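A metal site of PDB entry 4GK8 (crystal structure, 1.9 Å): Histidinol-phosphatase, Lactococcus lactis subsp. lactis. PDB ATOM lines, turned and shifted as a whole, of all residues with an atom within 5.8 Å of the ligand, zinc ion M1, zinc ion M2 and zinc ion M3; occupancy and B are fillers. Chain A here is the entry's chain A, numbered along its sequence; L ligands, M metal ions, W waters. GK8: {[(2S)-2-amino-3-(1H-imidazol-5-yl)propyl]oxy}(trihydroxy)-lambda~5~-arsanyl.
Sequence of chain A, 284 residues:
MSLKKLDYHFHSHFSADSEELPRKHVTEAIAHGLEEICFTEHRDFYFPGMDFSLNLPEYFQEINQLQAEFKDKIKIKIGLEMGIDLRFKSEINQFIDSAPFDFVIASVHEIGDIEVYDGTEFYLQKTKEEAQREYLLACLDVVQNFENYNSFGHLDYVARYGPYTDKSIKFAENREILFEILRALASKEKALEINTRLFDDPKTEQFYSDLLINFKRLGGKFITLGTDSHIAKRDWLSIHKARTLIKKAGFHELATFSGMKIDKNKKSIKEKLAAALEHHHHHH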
ATOM      1  N   HIS A   9      -1.664  -4.875   7.091  1.00  0.00           N
ATOM      2  CA  HIS A   9      -1.680  -3.434   7.335  1.00  0.00           C
ATOM      3  C   HIS A   9      -0.261  -2.959   7.638  1.00  0.00           C
ATOM      4  O   HIS A   9       0.259  -3.218   8.714  1.00  0.00           O
ATOM      5  CB  HIS A   9      -2.613  -3.082   8.507  1.00  0.00           C
ATOM      6  CG  HIS A   9      -2.859  -1.611   8.682  1.00  0.00           C
ATOM      7  ND1 HIS A   9      -3.984  -1.117   9.300  1.00  0.00           N
ATOM      8  CD2 HIS A   9      -2.132  -0.525   8.300  1.00  0.00           C
ATOM      9  CE1 HIS A   9      -3.928   0.209   9.311  1.00  0.00           C
ATOM     10  NE2 HIS A   9      -2.820   0.590   8.704  1.00  0.00           N
ATOM     11  N   PHE A  10       0.354  -2.274   6.677  1.00  0.00           N
ATOM     12  CA  PHE A  10       1.686  -1.696   6.902  1.00  0.00           C
ATOM     13  C   PHE A  10       2.025  -0.702   5.804  1.00  0.00           C
ATOM     14  O   PHE A  10       1.364  -0.652   4.753  1.00  0.00           O
ATOM     15  CB  PHE A  10       2.775  -2.790   7.069  1.00  0.00           C
ATOM     16  CG  PHE A  10       2.932  -3.693   5.871  1.00  0.00           C
ATOM     17  CD1 PHE A  10       3.855  -3.392   4.872  1.00  0.00           C
ATOM     18  CD2 PHE A  10       2.188  -4.859   5.764  1.00  0.00           C
ATOM     19  CE1 PHE A  10       4.009  -4.219   3.772  1.00  0.00           C
ATOM     20  CE2 PHE A  10       2.333  -5.686   4.675  1.00  0.00           C
ATOM     21  CZ  PHE A  10       3.248  -5.368   3.668  1.00  0.00           C
ATOM     22  N   HIS A  11       3.051   0.113   6.055  1.00  0.00           N
ATOM     23  CA  HIS A  11       3.334   1.288   5.239  1.00  0.00           C
ATOM     24  C   HIS A  11       4.797   1.383   4.846  1.00  0.00           C
ATOM     25  O   HIS A  11       5.678   1.026   5.639  1.00  0.00           O
ATOM     26  CB  HIS A  11       2.974   2.538   6.033  1.00  0.00           C
ATOM     27  CG  HIS A  11       1.539   2.580   6.465  1.00  0.00           C
ATOM     28  ND1 HIS A  11       0.562   3.199   5.720  1.00  0.00           N
ATOM     29  CD2 HIS A  11       0.916   2.078   7.553  1.00  0.00           C
ATOM     30  CE1 HIS A  11      -0.599   3.090   6.328  1.00  0.00           C
ATOM     31  NE2 HIS A  11      -0.416   2.407   7.445  1.00  0.00           N
ATOM     32  N   SER A  15       3.823   5.997   1.539  1.00  0.00           N
ATOM     33  CA  SER A  15       2.951   6.704   2.481  1.00  0.00           C
ATOM     34  C   SER A  15       3.633   7.951   2.999  1.00  0.00           C
ATOM     35  O   SER A  15       4.851   7.950   3.192  1.00  0.00           O
ATOM     36  CB  SER A  15       2.609   5.814   3.685  1.00  0.00           C
ATOM     37  OG  SER A  15       1.739   4.751   3.326  1.00  0.00           O
ATOM     38  N   ASP A  17       3.813   9.286   5.876  1.00  0.00           N
ATOM     39  CA  ASP A  17       4.409   9.245   7.207  1.00  0.00           C
ATOM     40  C   ASP A  17       5.325   8.030   7.415  1.00  0.00           C
ATOM     41  O   ASP A  17       5.557   7.614   8.547  1.00  0.00           O
ATOM     42  CB  ASP A  17       3.336   9.282   8.297  1.00  0.00           C
ATOM     43  CG  ASP A  17       2.434   8.062   8.290  1.00  0.00           C
ATOM     44  OD1 ASP A  17       2.485   7.301   7.313  1.00  0.00           O
ATOM     45  OD2 ASP A  17       1.638   7.869   9.264  1.00  0.00           O
ATOM     46  N   THR A  40      -0.487  -1.456   2.508  1.00  0.00           N
ATOM     47  CA  THR A  40      -1.703  -0.662   2.634  1.00  0.00           C
ATOM     48  C   THR A  40      -1.345   0.805   2.836  1.00  0.00           C
ATOM     49  O   THR A  40      -1.482   1.341   3.933  1.00  0.00           O
ATOM     50  CB  THR A  40      -2.617  -1.133   3.805  1.00  0.00           C
ATOM     51  OG1 THR A  40      -1.906  -1.068   5.036  1.00  0.00           O
ATOM     52  CG2 THR A  40      -3.117  -2.576   3.592  1.00  0.00           C
ATOM     53  N   HIS A  42      -1.131   4.969   2.734  1.00  0.00           N
ATOM     54  CA  HIS A  42      -2.106   6.031   3.051  1.00  0.00           C
ATOM     55  C   HIS A  42      -2.612   6.814   1.855  1.00  0.00           C
ATOM     56  O   HIS A  42      -1.805   7.323   1.048  1.00  0.00           O
ATOM     57  CB  HIS A  42      -1.445   7.083   3.959  1.00  0.00           C
ATOM     58  CG  HIS A  42      -1.293   6.668   5.396  1.00  0.00           C
ATOM     59  ND1 HIS A  42      -2.373   6.320   6.185  1.00  0.00           N
ATOM     60  CD2 HIS A  42      -0.203   6.611   6.191  1.00  0.00           C
ATOM     61  CE1 HIS A  42      -1.943   6.044   7.399  1.00  0.00           C
ATOM     62  NE2 HIS A  42      -0.636   6.216   7.430  1.00  0.00           N
ATOM     63  N   ASP A  44      -5.434  10.064   2.330  1.00  0.00           N
ATOM     64  CA  ASP A  44      -6.428  10.836   3.090  1.00  0.00           C
ATOM     65  C   ASP A  44      -6.618  12.162   2.336  1.00  0.00           C
ATOM     66  O   ASP A  44      -5.638  12.849   2.074  1.00  0.00           O
ATOM     67  CB  ASP A  44      -5.913  11.175   4.505  1.00  0.00           C
ATOM     68  CG  ASP A  44      -5.690   9.932   5.387  1.00  0.00           C
ATOM     69  OD1 ASP A  44      -4.655   9.242   5.203  1.00  0.00           O
ATOM     70  OD2 ASP A  44      -6.514   9.672   6.292  1.00  0.00           O
ATOM     71  N   PHE A  47      -6.213  16.423   4.145  1.00  0.00           N
ATOM     72  CA  PHE A  47      -5.888  16.127   5.531  1.00  0.00           C
ATOM     73  C   PHE A  47      -5.354  17.359   6.229  1.00  0.00           C
ATOM     74  O   PHE A  47      -4.598  18.114   5.631  1.00  0.00           O
ATOM     75  CB  PHE A  47      -4.867  14.993   5.650  1.00  0.00           C
ATOM     76  CG  PHE A  47      -4.865  14.313   6.994  1.00  0.00           C
ATOM     77  CD1 PHE A  47      -5.906  13.452   7.330  1.00  0.00           C
ATOM     78  CD2 PHE A  47      -3.875  14.566   7.925  1.00  0.00           C
ATOM     79  CE1 PHE A  47      -5.930  12.819   8.566  1.00  0.00           C
ATOM     80  CE2 PHE A  47      -3.890  13.941   9.169  1.00  0.00           C
ATOM     81  CZ  PHE A  47      -4.917  13.068   9.489  1.00  0.00           C
ATOM     82  N   MET A  50      -0.963  18.127   6.989  1.00  0.00           N
ATOM     83  CA  MET A  50      -0.006  17.282   6.293  1.00  0.00           C
ATOM     84  C   MET A  50      -0.681  16.528   5.157  1.00  0.00           C
ATOM     85  O   MET A  50      -1.751  15.953   5.336  1.00  0.00           O
ATOM     86  CB  MET A  50       0.584  16.285   7.289  1.00  0.00           C
ATOM     87  CG  MET A  50       1.529  15.260   6.683  1.00  0.00           C
ATOM     88  SD  MET A  50       2.120  14.177   7.998  1.00  0.00           S
ATOM     89  CE  MET A  50       3.108  13.035   7.051  1.00  0.00           C
ATOM     90  N   PHE A  52      -1.491  13.618   2.744  1.00  0.00           N
ATOM     91  CA  PHE A  52      -1.361  12.174   2.590  1.00  0.00           C
ATOM     92  C   PHE A  52      -1.763  11.772   1.181  1.00  0.00           C
ATOM     93  O   PHE A  52      -2.849  11.255   0.942  1.00  0.00           O
ATOM     94  CB  PHE A  52      -2.206  11.423   3.644  1.00  0.00           C
ATOM     95  CG  PHE A  52      -1.550  11.346   4.990  1.00  0.00           C
ATOM     96  CD1 PHE A  52      -0.752  10.262   5.326  1.00  0.00           C
ATOM     97  CD2 PHE A  52      -1.711  12.363   5.909  1.00  0.00           C
ATOM     98  CE1 PHE A  52      -0.146  10.186   6.563  1.00  0.00           C
ATOM     99  CE2 PHE A  52      -1.101  12.282   7.159  1.00  0.00           C
ATOM    100  CZ  PHE A  52      -0.317  11.199   7.483  1.00  0.00           C
ATOM    101  N   GLU A  81      -4.829   2.020   2.679  1.00  0.00           N
ATOM    102  CA  GLU A  81      -5.529   2.478   3.872  1.00  0.00           C
ATOM    103  C   GLU A  81      -6.153   3.818   3.556  1.00  0.00           C
ATOM    104  O   GLU A  81      -5.460   4.829   3.446  1.00  0.00           O
ATOM    105  CB  GLU A  81      -4.623   2.577   5.110  1.00  0.00           C
ATOM    106  CG  GLU A  81      -5.449   2.964   6.355  1.00  0.00           C
ATOM    107  CD  GLU A  81      -4.621   3.288   7.593  1.00  0.00           C
ATOM    108  OE1 GLU A  81      -3.381   3.318   7.533  1.00  0.00           O
ATOM    109  OE2 GLU A  81      -5.253   3.519   8.656  1.00  0.00           O
ATOM    110  N   SER A 107     -10.593   3.815   7.460  1.00  0.00           N
ATOM    111  CA  SER A 107     -10.117   4.284   8.752  1.00  0.00           C
ATOM    112  C   SER A 107     -10.638   5.686   9.010  1.00  0.00           C
ATOM    113  O   SER A 107     -10.857   6.456   8.074  1.00  0.00           O
ATOM    114  CB  SER A 107      -8.590   4.355   8.752  1.00  0.00           C
ATOM    115  OG  SER A 107      -8.004   3.061   8.753  1.00  0.00           O
ATOM    116  N   HIS A 109      -9.303   9.070  10.728  1.00  0.00           N
ATOM    117  CA  HIS A 109      -8.072   9.725  11.180  1.00  0.00           C
ATOM    118  C   HIS A 109      -8.289  11.183  11.568  1.00  0.00           C
ATOM    119  O   HIS A 109      -7.470  11.800  12.264  1.00  0.00           O
ATOM    120  CB  HIS A 109      -7.004   9.671  10.086  1.00  0.00           C
ATOM    121  CG  HIS A 109      -6.499   8.295   9.795  1.00  0.00           C
ATOM    122  ND1 HIS A 109      -6.244   7.853   8.516  1.00  0.00           N
ATOM    123  CD2 HIS A 109      -6.193   7.256  10.621  1.00  0.00           C
ATOM    124  CE1 HIS A 109      -5.809   6.603   8.562  1.00  0.00           C
ATOM    125  NE2 HIS A 109      -5.763   6.216   9.822  1.00  0.00           N
ATOM    126  N   GLU A 115      -7.438  16.664  13.383  1.00  0.00           N
ATOM    127  CA  GLU A 115      -6.791  15.359  13.400  1.00  0.00           C
ATOM    128  C   GLU A 115      -6.861  14.682  14.774  1.00  0.00           C
ATOM    129  O   GLU A 115      -6.656  15.315  15.809  1.00  0.00           O
ATOM    130  CB  GLU A 115      -5.320  15.470  12.956  1.00  0.00           C
ATOM    131  CG  GLU A 115      -4.603  14.132  12.987  1.00  0.00           C
ATOM    132  CD  GLU A 115      -3.140  14.227  12.594  1.00  0.00           C
ATOM    133  OE1 GLU A 115      -2.596  15.339  12.548  1.00  0.00           O
ATOM    134  OE2 GLU A 115      -2.548  13.164  12.330  1.00  0.00           O
ATOM    135  N   VAL A 116      -7.180  13.395  14.778  1.00  0.00           N
ATOM    136  CA  VAL A 116      -7.132  12.599  15.998  1.00  0.00           C
ATOM    137  C   VAL A 116      -5.683  12.141  16.174  1.00  0.00           C
ATOM    138  O   VAL A 116      -5.238  11.204  15.515  1.00  0.00           O
ATOM    139  CB  VAL A 116      -8.094  11.387  15.910  1.00  0.00           C
ATOM    140  CG1 VAL A 116      -8.080  10.580  17.223  1.00  0.00           C
ATOM    141  CG2 VAL A 116      -9.502  11.865  15.574  1.00  0.00           C
ATOM    142  N   TYR A 117      -4.933  12.812  17.041  1.00  0.00           N
ATOM    143  CA  TYR A 117      -3.507  12.552  17.152  1.00  0.00           C
ATOM    144  C   TYR A 117      -2.958  13.268  18.360  1.00  0.00           C
ATOM    145  O   TYR A 117      -3.638  14.103  18.930  1.00  0.00           O
ATOM    146  CB  TYR A 117      -2.770  13.021  15.894  1.00  0.00           C
ATOM    147  CG  TYR A 117      -1.448  12.308  15.678  1.00  0.00           C
ATOM    148  CD1 TYR A 117      -1.421  10.982  15.253  1.00  0.00           C
ATOM    149  CD2 TYR A 117      -0.237  12.962  15.879  1.00  0.00           C
ATOM    150  CE1 TYR A 117      -0.223  10.312  15.050  1.00  0.00           C
ATOM    151  CE2 TYR A 117       0.970  12.296  15.675  1.00  0.00           C
ATOM    152  CZ  TYR A 117       0.966  10.975  15.269  1.00  0.00           C
ATOM    153  OH  TYR A 117       2.151  10.306  15.055  1.00  0.00           O
ATOM    154  N   HIS A 154      -8.418  -0.216  12.766  1.00  0.00           N
ATOM    155  CA  HIS A 154      -8.159   0.182  14.154  1.00  0.00           C
ATOM    156  C   HIS A 154      -9.271   0.923  14.915  1.00  0.00           C
ATOM    157  O   HIS A 154      -9.238   2.138  15.051  1.00  0.00           O
ATOM    158  CB  HIS A 154      -6.825   0.977  14.251  1.00  0.00           C
ATOM    159  CG  HIS A 154      -6.693   2.101  13.260  1.00  0.00           C
ATOM    160  ND1 HIS A 154      -7.685   3.034  13.032  1.00  0.00           N
ATOM    161  CD2 HIS A 154      -5.670   2.448  12.449  1.00  0.00           C
ATOM    162  CE1 HIS A 154      -7.268   3.912  12.128  1.00  0.00           C
ATOM    163  NE2 HIS A 154      -6.047   3.582  11.755  1.00  0.00           N
ATOM    164  N   TYR A 157      -8.058   3.244  17.641  1.00  0.00           N
ATOM    165  CA  TYR A 157      -7.147   4.317  17.222  1.00  0.00           C
ATOM    166  C   TYR A 157      -7.101   5.478  18.221  1.00  0.00           C
ATOM    167  O   TYR A 157      -6.029   6.011  18.540  1.00  0.00           O
ATOM    168  CB  TYR A 157      -7.555   4.822  15.831  1.00  0.00           C
ATOM    169  CG  TYR A 157      -6.623   5.819  15.162  1.00  0.00           C
ATOM    170  CD1 TYR A 157      -5.466   5.397  14.513  1.00  0.00           C
ATOM    171  CD2 TYR A 157      -6.949   7.177  15.113  1.00  0.00           C
ATOM    172  CE1 TYR A 157      -4.638   6.308  13.869  1.00  0.00           C
ATOM    173  CE2 TYR A 157      -6.121   8.093  14.478  1.00  0.00           C
ATOM    174  CZ  TYR A 157      -4.971   7.646  13.862  1.00  0.00           C
ATOM    175  OH  TYR A 157      -4.148   8.550  13.232  1.00  0.00           O
ATOM    176  N   ARG A 160      -4.673   5.460  21.145  1.00  0.00           N
ATOM    177  CA  ARG A 160      -3.235   5.599  20.962  1.00  0.00           C
ATOM    178  C   ARG A 160      -2.737   6.933  21.496  1.00  0.00           C
ATOM    179  O   ARG A 160      -1.572   7.056  21.863  1.00  0.00           O
ATOM    180  CB  ARG A 160      -2.849   5.491  19.495  1.00  0.00           C
ATOM    181  CG  ARG A 160      -3.209   4.163  18.828  1.00  0.00           C
ATOM    182  CD  ARG A 160      -2.971   4.305  17.327  1.00  0.00           C
ATOM    183  NE  ARG A 160      -3.147   3.042  16.612  1.00  0.00           N
ATOM    184  CZ  ARG A 160      -2.782   2.880  15.342  1.00  0.00           C
ATOM    185  NH1 ARG A 160      -2.226   3.904  14.703  1.00  0.00           N
ATOM    186  NH2 ARG A 160      -2.953   1.706  14.741  1.00  0.00           N
ATOM    187  N   TYR A 161      -3.598   7.938  21.510  1.00  0.00           N
ATOM    188  CA  TYR A 161      -3.121   9.319  21.631  1.00  0.00           C
ATOM    189  C   TYR A 161      -3.874  10.079  22.702  1.00  0.00           C
ATOM    190  O   TYR A 161      -4.856   9.598  23.245  1.00  0.00           O
ATOM    191  CB  TYR A 161      -3.245  10.062  20.291  1.00  0.00           C
ATOM    192  CG  TYR A 161      -2.801   9.254  19.086  1.00  0.00           C
ATOM    193  CD1 TYR A 161      -1.451   8.993  18.870  1.00  0.00           C
ATOM    194  CD2 TYR A 161      -3.733   8.752  18.176  1.00  0.00           C
ATOM    195  CE1 TYR A 161      -1.033   8.238  17.761  1.00  0.00           C
ATOM    196  CE2 TYR A 161      -3.324   7.997  17.078  1.00  0.00           C
ATOM    197  CZ  TYR A 161      -1.978   7.753  16.876  1.00  0.00           C
ATOM    198  OH  TYR A 161      -1.570   7.003  15.788  1.00  0.00           O
ATOM    199  N   ASN A 195      -5.816  -4.851  14.890  1.00  0.00           N
ATOM    200  CA  ASN A 195      -4.633  -4.019  14.687  1.00  0.00           C
ATOM    201  C   ASN A 195      -3.708  -4.178  15.885  1.00  0.00           C
ATOM    202  O   ASN A 195      -4.112  -3.919  17.013  1.00  0.00           O
ATOM    203  CB  ASN A 195      -5.075  -2.551  14.524  1.00  0.00           C
ATOM    204  CG  ASN A 195      -3.939  -1.646  14.081  1.00  0.00           C
ATOM    205  OD1 ASN A 195      -2.892  -1.576  14.722  1.00  0.00           O
ATOM    206  ND2 ASN A 195      -4.148  -0.945  12.977  1.00  0.00           N
ATOM    207  N   ARG A 197      -0.952  -2.611  16.876  1.00  0.00           N
ATOM    208  CA  ARG A 197      -0.130  -1.481  17.304  1.00  0.00           C
ATOM    209  C   ARG A 197       0.059  -1.400  18.830  1.00  0.00           C
ATOM    210  O   ARG A 197       1.192  -1.317  19.302  1.00  0.00           O
ATOM    211  CB  ARG A 197      -0.667  -0.152  16.765  1.00  0.00           C
ATOM    212  CG  ARG A 197       0.057   1.080  17.366  1.00  0.00           C
ATOM    213  CD  ARG A 197       1.500   1.242  16.878  1.00  0.00           C
ATOM    214  NE  ARG A 197       1.553   1.462  15.430  1.00  0.00           N
ATOM    215  CZ  ARG A 197       1.260   2.620  14.835  1.00  0.00           C
ATOM    216  NH1 ARG A 197       0.900   3.670  15.554  1.00  0.00           N
ATOM    217  NH2 ARG A 197       1.307   2.713  13.508  1.00  0.00           N
ATOM    218  N   ASP A 228       0.304  -2.507  11.394  1.00  0.00           N
ATOM    219  CA  ASP A 228       0.399  -1.059  11.210  1.00  0.00           C
ATOM    220  C   ASP A 228       1.853  -0.556  11.271  1.00  0.00           C
ATOM    221  O   ASP A 228       2.109   0.584  11.648  1.00  0.00           O
ATOM    222  CB  ASP A 228      -0.459  -0.301  12.227  1.00  0.00           C
ATOM    223  CG  ASP A 228      -1.157   0.911  11.618  1.00  0.00           C
ATOM    224  OD1 ASP A 228      -0.724   1.406  10.553  1.00  0.00           O
ATOM    225  OD2 ASP A 228      -2.150   1.362  12.212  1.00  0.00           O
ATOM    226  N   HIS A 230       5.315   1.006  10.282  1.00  0.00           N
ATOM    227  CA  HIS A 230       5.802   1.996   9.341  1.00  0.00           C
ATOM    228  C   HIS A 230       7.294   1.773   9.087  1.00  0.00           C
ATOM    229  O   HIS A 230       7.900   2.461   8.277  1.00  0.00           O
ATOM    230  CB  HIS A 230       5.535   3.411   9.846  1.00  0.00           C
ATOM    231  CG  HIS A 230       4.076   3.770   9.833  1.00  0.00           C
ATOM    232  ND1 HIS A 230       3.122   3.008  10.466  1.00  0.00           N
ATOM    233  CD2 HIS A 230       3.421   4.804   9.259  1.00  0.00           C
ATOM    234  CE1 HIS A 230       1.938   3.563  10.282  1.00  0.00           C
ATOM    235  NE2 HIS A 230       2.092   4.658   9.555  1.00  0.00           N
HETATM  236  C   GK8 L   1      -1.046   7.681  11.447  1.00  0.00           C
HETATM  237  N   GK8 L   1      -2.947   8.505  10.204  1.00  0.00           N
HETATM  238 AS   GK8 L   1      -1.614   5.039  10.927  1.00  0.00          AS
HETATM  239  O1  GK8 L   1      -1.236   4.426  12.539  1.00  0.00           O
HETATM  240  O2  GK8 L   1      -3.274   5.667  10.742  1.00  0.00           O
HETATM  241  O3  GK8 L   1      -1.116   4.049   9.551  1.00  0.00           O
HETATM  242  O4  GK8 L   1      -0.610   6.528  10.818  1.00  0.00           O
HETATM  243  CA  GK8 L   1      -1.595   8.798  10.596  1.00  0.00           C
HETATM  244  CB  GK8 L   1      -1.568  10.114  11.321  1.00  0.00           C
HETATM  245  CG  GK8 L   1      -0.308  10.919  11.326  1.00  0.00           C
HETATM  246  ND1 GK8 L   1      -0.195  12.251  11.564  1.00  0.00           N
HETATM  247  CD2 GK8 L   1       0.988  10.456  11.088  1.00  0.00           C
HETATM  248  CE1 GK8 L   1       1.089  12.602  11.484  1.00  0.00           C
HETATM  249  NE2 GK8 L   1       1.806  11.516  11.198  1.00  0.00           N
HETATM  250 ZN    ZN M   1      -4.745   4.477  10.325  1.00  0.00          ZN
HETATM  251 ZN    ZN M   2       0.603   6.065   9.096  1.00  0.00          ZN
HETATM  252 ZN    ZN M   3      -1.925   2.499   8.989  1.00  0.00          ZN
HETATM  253  O   HOH W   1      -3.303   3.014  10.492  1.00  0.00           O
HETATM  254  O   HOH W   2      -3.313   9.456   7.834  1.00  0.00           O
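A ring nitrogen (ND1) of His 42 lies close to the side-chain carboxylate of Glu 81 (3.4 Å). ND1 of His 109 lies within hydrogen-bond range of OD2 of Asp 44 (2.9 Å). ND1 of His 230 lies within hydrogen-bond range of O of Asp 228, at 2.9 Å. A ring nitrogen (ND1) of His 11 lies within hydrogen-bond range of the side-chain hydroxyl (OG) of Ser 15. NH2 of Arg 160 is in salt-bridge range of OD2 of Asp 228 (2.7 Å). The guanidinium group (NH1) of Arg 160 is in hydrogen-bond range of the side-chain hydroxyl (OH) of Tyr 161 (3.3 Å). The backbone NH of Arg 197 lies within hydrogen-bond range of the side-chain amide oxygen of Asn 195 (3.1 Å). O of Phe 52 lies within hydrogen-bond range of N of Asp 44 (3.2 Å).
Zinc ion M3 is bound by an oxygen (O3) of the ligand (1.8 Å), water W1 (2.1 Å), a ring nitrogen (NE2) of His 9 (2.1 Å), a ring nitrogen (NE2) of His 11 (2.2 Å), the side-chain carboxylate of Glu 81 (2.2 Å) and the side-chain carboxylate of Asp 228 (2.3 Å). Zinc ion M3 has six donor atoms within binding distance.
Residues that only touch zinc ion M1: Ser 107 (3.9 Å) and Tyr 157 (3.99 Å). The nearest printed residue that does not touch zinc ion M1 is His 42 (4.3 Å).
Water W1 lies within hydrogen-bond range of the side-chain carboxylate (OD2) of Asp 228 (2.6 Å) and an oxygen (O1) of the ligand (3.2 Å). Water W2 lies within hydrogen-bond range of a nitrogen (N) of the ligand (2.6 Å), the side-chain carboxylate (OD1) of Asp 44 (3.0 Å) and a ring nitrogen (ND1) of His 109 (3.4 Å).
Met 50 touches the ligand (SD to CE1, 3.96 Å). Phe 52 touches the ligand (CZ to CG, 3.9 Å). CE1 of Tyr 117 touches CG of the ligand, 3.8 Å away. Hydrophobic or aromatic side chains within 4 Å of the ligand: His 11, His 42, Met 50, Phe 52, His 109, Tyr 117, Tyr 157 and His 230. Of the 25 residues printed, 16 come within 4 Å of the ligand. The nearest printed residue that does not touch the ligand is Tyr 161 (4.2 Å).
Zinc ion M1 is bound by O2 of the ligand (1.9 Å), OE2 of Glu 81 (2.0 Å), water W1 (2.1 Å), NE2 of His 109 (2.1 Å) and NE2 of His 154 (2.1 Å). Zinc ion M1 has five donor atoms within binding distance.
Of the 25 residues printed, 3 come within 4 Å of zinc ion M2. The nearest printed residue that does not touch zinc ion M2 is His 11 (4.1 Å).
Of the 25 residues printed, 5 come within 4 Å of zinc ion M3. The nearest printed residue that does not touch zinc ion M3 is His 230 (4.2 Å).
The guanidinium group (NH1) of Arg 160 sits at hydrogen-bond distance from an oxygen (O1) of the ligand. The side-chain carboxylate (OE2) of Glu 115 sits at hydrogen-bond distance from a nitrogen (ND1) of the ligand (2.6 Å). An oxygen (O1) of the ligand is in hydrogen-bond range of the guanidinium group (NH2) of Arg 197 (3.2 Å). The side-chain hydroxyl of Tyr 157 is in hydrogen-bond range of a nitrogen (N) of the ligand (3.3 Å).
Zinc ion M2 is bound by NE2 of His 42, OD2 of Asp 17, NE2 of His 230 and O4 of the ligand. Zinc ion M2 has four donor atoms within binding distance. Slightly farther from zinc ion M2 lies O3 of the ligand (2.7 Å).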
